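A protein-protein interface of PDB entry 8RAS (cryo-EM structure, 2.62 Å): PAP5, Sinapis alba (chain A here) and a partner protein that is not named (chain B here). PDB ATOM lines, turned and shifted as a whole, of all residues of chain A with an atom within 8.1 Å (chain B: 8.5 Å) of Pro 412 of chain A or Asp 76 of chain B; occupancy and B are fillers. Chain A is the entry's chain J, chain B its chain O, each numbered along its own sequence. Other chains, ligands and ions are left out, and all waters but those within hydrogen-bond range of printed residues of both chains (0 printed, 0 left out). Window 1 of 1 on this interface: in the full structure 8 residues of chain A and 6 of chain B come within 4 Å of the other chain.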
ATOM      1  N   PHE A 404     -22.402  11.020 -21.056  1.00  0.00           N
ATOM      2  CA  PHE A 404     -21.327  10.410 -21.824  1.00  0.00           C
ATOM      3  C   PHE A 404     -21.755   9.999 -23.224  1.00  0.00           C
ATOM      4  O   PHE A 404     -20.917   9.522 -23.995  1.00  0.00           O
ATOM      5  CB  PHE A 404     -20.770   9.206 -21.065  1.00  0.00           C
ATOM      6  CG  PHE A 404     -20.005   9.578 -19.829  1.00  0.00           C
ATOM      7  CD1 PHE A 404     -19.191  10.696 -19.818  1.00  0.00           C
ATOM      8  CD2 PHE A 404     -20.106   8.817 -18.679  1.00  0.00           C
ATOM      9  CE1 PHE A 404     -18.486  11.044 -18.685  1.00  0.00           C
ATOM     10  CE2 PHE A 404     -19.403   9.161 -17.543  1.00  0.00           C
ATOM     11  CZ  PHE A 404     -18.593  10.276 -17.546  1.00  0.00           C
ATOM     12  N   ARG A 405     -23.027  10.173 -23.570  1.00  0.00           N
ATOM     13  CA  ARG A 405     -23.515   9.944 -24.922  1.00  0.00           C
ATOM     14  C   ARG A 405     -23.654  11.238 -25.713  1.00  0.00           C
ATOM     15  O   ARG A 405     -24.291  11.240 -26.770  1.00  0.00           O
ATOM     16  CB  ARG A 405     -24.854   9.207 -24.885  1.00  0.00           C
ATOM     17  CG  ARG A 405     -24.769   7.796 -24.333  1.00  0.00           C
ATOM     18  CD  ARG A 405     -23.653   7.007 -24.996  1.00  0.00           C
ATOM     19  NE  ARG A 405     -23.793   6.965 -26.445  1.00  0.00           N
ATOM     20  CZ  ARG A 405     -24.622   6.161 -27.097  1.00  0.00           C
ATOM     21  NH1 ARG A 405     -25.404   5.309 -26.456  1.00  0.00           N
ATOM     22  NH2 ARG A 405     -24.664   6.211 -28.425  1.00  0.00           N
ATOM     23  N   PHE A 409     -18.287  13.207 -27.060  1.00  0.00           N
ATOM     24  CA  PHE A 409     -17.719  11.979 -26.532  1.00  0.00           C
ATOM     25  C   PHE A 409     -17.603  10.933 -27.630  1.00  0.00           C
ATOM     26  O   PHE A 409     -18.388  10.915 -28.581  1.00  0.00           O
ATOM     27  CB  PHE A 409     -18.569  11.425 -25.384  1.00  0.00           C
ATOM     28  CG  PHE A 409     -18.418  12.183 -24.103  1.00  0.00           C
ATOM     29  CD1 PHE A 409     -17.381  11.898 -23.234  1.00  0.00           C
ATOM     30  CD2 PHE A 409     -19.310  13.184 -23.768  1.00  0.00           C
ATOM     31  CE1 PHE A 409     -17.238  12.595 -22.057  1.00  0.00           C
ATOM     32  CE2 PHE A 409     -19.172  13.884 -22.594  1.00  0.00           C
ATOM     33  CZ  PHE A 409     -18.136  13.589 -21.736  1.00  0.00           C
ATOM     34  N   HIS A 410     -16.611  10.060 -27.484  1.00  0.00           N
ATOM     35  CA  HIS A 410     -16.450   8.943 -28.398  1.00  0.00           C
ATOM     36  C   HIS A 410     -17.549   7.908 -28.165  1.00  0.00           C
ATOM     37  O   HIS A 410     -18.348   8.004 -27.230  1.00  0.00           O
ATOM     38  CB  HIS A 410     -15.072   8.305 -28.228  1.00  0.00           C
ATOM     39  CG  HIS A 410     -14.792   7.835 -26.835  1.00  0.00           C
ATOM     40  ND1 HIS A 410     -15.279   6.647 -26.337  1.00  0.00           N
ATOM     41  CD2 HIS A 410     -14.072   8.394 -25.833  1.00  0.00           C
ATOM     42  CE1 HIS A 410     -14.875   6.494 -25.089  1.00  0.00           C
ATOM     43  NE2 HIS A 410     -14.141   7.541 -24.759  1.00  0.00           N
ATOM     44  N   GLU A 411     -17.583   6.908 -29.038  1.00  0.00           N
ATOM     45  CA  GLU A 411     -18.548   5.834 -28.894  1.00  0.00           C
ATOM     46  C   GLU A 411     -18.247   5.030 -27.630  1.00  0.00           C
ATOM     47  O   GLU A 411     -17.095   4.957 -27.195  1.00  0.00           O
ATOM     48  CB  GLU A 411     -18.517   4.922 -30.115  1.00  0.00           C
ATOM     49  CG  GLU A 411     -19.020   5.577 -31.389  1.00  0.00           C
ATOM     50  CD  GLU A 411     -20.331   6.306 -31.189  1.00  0.00           C
ATOM     51  OE1 GLU A 411     -21.378   5.636 -31.097  1.00  0.00           O
ATOM     52  OE2 GLU A 411     -20.314   7.553 -31.125  1.00  0.00           O
ATOM     53  N   PRO A 412     -19.269   4.440 -27.010  1.00  0.00           N
ATOM     54  CA  PRO A 412     -19.036   3.657 -25.790  1.00  0.00           C
ATOM     55  C   PRO A 412     -18.010   2.557 -26.021  1.00  0.00           C
ATOM     56  O   PRO A 412     -18.084   1.809 -26.999  1.00  0.00           O
ATOM     57  CB  PRO A 412     -20.420   3.083 -25.471  1.00  0.00           C
ATOM     58  CG  PRO A 412     -21.374   4.033 -26.097  1.00  0.00           C
ATOM     59  CD  PRO A 412     -20.701   4.562 -27.329  1.00  0.00           C
ATOM     60  N   THR A 413     -17.051   2.468 -25.112  1.00  0.00           N
ATOM     61  CA  THR A 413     -15.979   1.489 -25.241  1.00  0.00           C
ATOM     62  C   THR A 413     -16.523   0.094 -24.972  1.00  0.00           C
ATOM     63  O   THR A 413     -17.067  -0.150 -23.887  1.00  0.00           O
ATOM     64  CB  THR A 413     -14.844   1.809 -24.275  1.00  0.00           C
ATOM     65  OG1 THR A 413     -14.207   3.030 -24.670  1.00  0.00           O
ATOM     66  CG2 THR A 413     -13.816   0.691 -24.273  1.00  0.00           C
ATOM     67  N   PRO A 414     -16.404  -0.841 -25.908  1.00  0.00           N
ATOM     68  CA  PRO A 414     -16.925  -2.188 -25.680  1.00  0.00           C
ATOM     69  C   PRO A 414     -16.024  -2.995 -24.759  1.00  0.00           C
ATOM     70  O   PRO A 414     -14.826  -2.739 -24.624  1.00  0.00           O
ATOM     71  CB  PRO A 414     -16.955  -2.793 -27.087  1.00  0.00           C
ATOM     72  CG  PRO A 414     -15.849  -2.098 -27.802  1.00  0.00           C
ATOM     73  CD  PRO A 414     -15.760  -0.708 -27.227  1.00  0.00           C
ATOM     74  N   ASN A 415     -16.636  -3.981 -24.107  1.00  0.00           N
ATOM     75  CA  ASN A 415     -15.877  -4.932 -23.309  1.00  0.00           C
ATOM     76  C   ASN A 415     -14.911  -5.686 -24.216  1.00  0.00           C
ATOM     77  O   ASN A 415     -15.296  -6.159 -25.288  1.00  0.00           O
ATOM     78  CB  ASN A 415     -16.831  -5.901 -22.609  1.00  0.00           C
ATOM     79  CG  ASN A 415     -16.181  -6.649 -21.457  1.00  0.00           C
ATOM     80  OD1 ASN A 415     -16.857  -7.350 -20.705  1.00  0.00           O
ATOM     81  ND2 ASN A 415     -14.875  -6.486 -21.298  1.00  0.00           N
ATOM     82  N   VAL B  73     -22.203  -7.664 -27.917  1.00  0.00           N
ATOM     83  CA  VAL B  73     -22.106  -6.223 -27.716  1.00  0.00           C
ATOM     84  C   VAL B  73     -23.428  -5.596 -28.134  1.00  0.00           C
ATOM     85  O   VAL B  73     -23.864  -5.751 -29.281  1.00  0.00           O
ATOM     86  CB  VAL B  73     -20.933  -5.618 -28.503  1.00  0.00           C
ATOM     87  CG1 VAL B  73     -20.874  -4.114 -28.296  1.00  0.00           C
ATOM     88  CG2 VAL B  73     -19.623  -6.270 -28.086  1.00  0.00           C
ATOM     89  N   ARG B  74     -24.063  -4.892 -27.203  1.00  0.00           N
ATOM     90  CA  ARG B  74     -25.306  -4.190 -27.490  1.00  0.00           C
ATOM     91  C   ARG B  74     -25.056  -3.044 -28.464  1.00  0.00           C
ATOM     92  O   ARG B  74     -23.994  -2.417 -28.462  1.00  0.00           O
ATOM     93  CB  ARG B  74     -25.911  -3.653 -26.192  1.00  0.00           C
ATOM     94  CG  ARG B  74     -27.349  -3.171 -26.284  1.00  0.00           C
ATOM     95  CD  ARG B  74     -28.283  -4.254 -26.791  1.00  0.00           C
ATOM     96  NE  ARG B  74     -29.677  -3.926 -26.514  1.00  0.00           N
ATOM     97  CZ  ARG B  74     -30.616  -3.793 -27.439  1.00  0.00           C
ATOM     98  NH1 ARG B  74     -30.352  -3.966 -28.722  1.00  0.00           N
ATOM     99  NH2 ARG B  74     -31.854  -3.482 -27.066  1.00  0.00           N
ATOM    100  N   GLU B  75     -26.044  -2.778 -29.313  1.00  0.00           N
ATOM    101  CA  GLU B  75     -25.946  -1.650 -30.228  1.00  0.00           C
ATOM    102  C   GLU B  75     -26.187  -0.340 -29.488  1.00  0.00           C
ATOM    103  O   GLU B  75     -26.981  -0.267 -28.546  1.00  0.00           O
ATOM    104  CB  GLU B  75     -26.937  -1.793 -31.383  1.00  0.00           C
ATOM    105  CG  GLU B  75     -28.356  -2.121 -30.963  1.00  0.00           C
ATOM    106  CD  GLU B  75     -28.725  -3.560 -31.264  1.00  0.00           C
ATOM    107  OE1 GLU B  75     -27.819  -4.347 -31.612  1.00  0.00           O
ATOM    108  OE2 GLU B  75     -29.921  -3.903 -31.153  1.00  0.00           O
ATOM    109  N   ASP B  76     -25.484   0.703 -29.929  1.00  0.00           N
ATOM    110  CA  ASP B  76     -25.519   1.987 -29.241  1.00  0.00           C
ATOM    111  C   ASP B  76     -26.742   2.823 -29.590  1.00  0.00           C
ATOM    112  O   ASP B  76     -27.032   3.791 -28.879  1.00  0.00           O
ATOM    113  CB  ASP B  76     -24.253   2.783 -29.561  1.00  0.00           C
ATOM    114  CG  ASP B  76     -23.005   2.142 -28.997  1.00  0.00           C
ATOM    115  OD1 ASP B  76     -23.011   1.784 -27.803  1.00  0.00           O
ATOM    116  OD2 ASP B  76     -22.016   1.996 -29.746  1.00  0.00           O
ATOM    117  N   TYR B  77     -27.462   2.483 -30.656  1.00  0.00           N
ATOM    118  CA  TYR B  77     -28.584   3.286 -31.123  1.00  0.00           C
ATOM    119  C   TYR B  77     -29.791   2.392 -31.353  1.00  0.00           C
ATOM    120  O   TYR B  77     -29.679   1.344 -31.997  1.00  0.00           O
ATOM    121  CB  TYR B  77     -28.219   4.040 -32.404  1.00  0.00           C
ATOM    122  CG  TYR B  77     -26.951   4.849 -32.268  1.00  0.00           C
ATOM    123  CD1 TYR B  77     -26.976   6.127 -31.730  1.00  0.00           C
ATOM    124  CD2 TYR B  77     -25.728   4.327 -32.661  1.00  0.00           C
ATOM    125  CE1 TYR B  77     -25.819   6.865 -31.594  1.00  0.00           C
ATOM    126  CE2 TYR B  77     -24.567   5.057 -32.529  1.00  0.00           C
ATOM    127  CZ  TYR B  77     -24.618   6.325 -31.996  1.00  0.00           C
ATOM    128  OH  TYR B  77     -23.461   7.055 -31.866  1.00  0.00           O
ATOM    129  N   LEU B  78     -30.942   2.810 -30.827  1.00  0.00           N
ATOM    130  CA  LEU B  78     -32.174   2.045 -30.951  1.00  0.00           C
ATOM    131  C   LEU B  78     -33.105   2.568 -32.035  1.00  0.00           C
ATOM    132  O   LEU B  78     -34.003   1.836 -32.461  1.00  0.00           O
ATOM    133  CB  LEU B  78     -32.927   2.032 -29.616  1.00  0.00           C
ATOM    134  CG  LEU B  78     -32.194   1.424 -28.420  1.00  0.00           C
ATOM    135  CD1 LEU B  78     -33.084   1.443 -27.193  1.00  0.00           C
ATOM    136  CD2 LEU B  78     -31.737   0.012 -28.735  1.00  0.00           C
ATOM    137  N   VAL B  79     -32.918   3.805 -32.483  1.00  0.00           N
ATOM    138  CA  VAL B  79     -33.763   4.373 -33.526  1.00  0.00           C
ATOM    139  C   VAL B  79     -33.243   3.918 -34.882  1.00  0.00           C
ATOM    140  O   VAL B  79     -32.067   4.112 -35.209  1.00  0.00           O
ATOM    141  CB  VAL B  79     -33.797   5.905 -33.424  1.00  0.00           C
ATOM    142  CG1 VAL B  79     -34.619   6.496 -34.556  1.00  0.00           C
ATOM    143  CG2 VAL B  79     -34.356   6.331 -32.078  1.00  0.00           C
ATOM    144  N   ARG B  80     -34.120   3.309 -35.673  1.00  0.00           N
ATOM    145  CA  ARG B  80     -33.751   2.731 -36.956  1.00  0.00           C
ATOM    146  C   ARG B  80     -34.068   3.698 -38.087  1.00  0.00           C
ATOM    147  O   ARG B  80     -35.083   4.399 -38.054  1.00  0.00           O
ATOM    148  CB  ARG B  80     -34.482   1.406 -37.184  1.00  0.00           C
ATOM    149  CG  ARG B  80     -33.560   0.238 -37.480  1.00  0.00           C
ATOM    150  CD  ARG B  80     -32.579   0.016 -36.343  1.00  0.00           C
ATOM    151  NE  ARG B  80     -33.250  -0.395 -35.116  1.00  0.00           N
ATOM    152  CZ  ARG B  80     -32.623  -0.795 -34.018  1.00  0.00           C
ATOM    153  NH1 ARG B  80     -31.303  -0.851 -33.957  1.00  0.00           N
ATOM    154  NH2 ARG B  80     -33.340  -1.147 -32.955  1.00  0.00           N
ATOM    155  N   GLU B 119     -33.403   9.141 -28.948  1.00  0.00           N
ATOM    156  CA  GLU B 119     -32.776   7.966 -28.352  1.00  0.00           C
ATOM    157  C   GLU B 119     -33.270   7.751 -26.926  1.00  0.00           C
ATOM    158  O   GLU B 119     -33.584   6.620 -26.529  1.00  0.00           O
ATOM    159  CB  GLU B 119     -31.256   8.109 -28.382  1.00  0.00           C
ATOM    160  CG  GLU B 119     -30.638   7.817 -29.734  1.00  0.00           C
ATOM    161  CD  GLU B 119     -30.707   6.350 -30.099  1.00  0.00           C
ATOM    162  OE1 GLU B 119     -30.715   5.506 -29.178  1.00  0.00           O
ATOM    163  OE2 GLU B 119     -30.758   6.041 -31.306  1.00  0.00           O
ATOM    164  N   VAL B 123     -35.482   4.575 -25.522  1.00  0.00           N
ATOM    165  CA  VAL B 123     -35.165   3.841 -24.301  1.00  0.00           C
ATOM    166  C   VAL B 123     -36.373   3.809 -23.373  1.00  0.00           C
ATOM    167  O   VAL B 123     -36.655   2.792 -22.728  1.00  0.00           O
ATOM    168  CB  VAL B 123     -33.932   4.450 -23.608  1.00  0.00           C
ATOM    169  CG1 VAL B 123     -33.721   3.818 -22.245  1.00  0.00           C
ATOM    170  CG2 VAL B 123     -32.698   4.268 -24.472  1.00  0.00           C
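The backbone carbonyl oxygen (O) of Asp 76 of chain B lies within hydrogen-bond range of the guanidinium group (NH1) of Arg 405 of chain A (3.3 Å).
The side-chain carboxylate (OE1) of Glu 411 of chain A sits at hydrogen-bond distance from the side-chain hydroxyl (OH) of Tyr 77 of chain B.
NH1 of Arg 80 of chain B is in hydrogen-bond range of O of Tyr 77 of chain B (3.4 Å).
Among the printed residues, pairs that only touch across the chains: Pro 412 of chain A with Asp 76 of chain B (3.3 Å), Arg 405 of chain A with Tyr 77 of chain B (3.4 Å) and Glu 411 of chain A with Asp 76 of chain B (3.9 Å).
Of the printed residues of chain B, Arg 405 of chain A touches Asp 76 and Tyr 77.
Of the printed residues of chain B, Glu 411 of chain A touches Asp 76 (3.9 Å) and Tyr 77 (2.6 Å).
Pro 412 of chain A touches just one residue of chain B: Asp 76.
Printed residues of chain A within 4 Å of Tyr 77 of chain B: Arg 405 (3.4 Å) and Glu 411 (2.6 Å).
The nearest residue of chain A that does not touch Asp 76 of chain B is Thr 413 of chain A (6.6 Å).
The nearest printed residue of chain B that does not touch Glu 411 of chain A is Glu 75 of chain B (7.8 Å).
Printed residues of chain B that touch a printed residue of chain A: Asp 76 and Tyr 77.
Hydrophobic or aromatic side chains of chain B that line the printed part of chain A: Tyr 77.
Along chain B the printed residues that touch a printed residue of chain A span positions 76 to 77.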
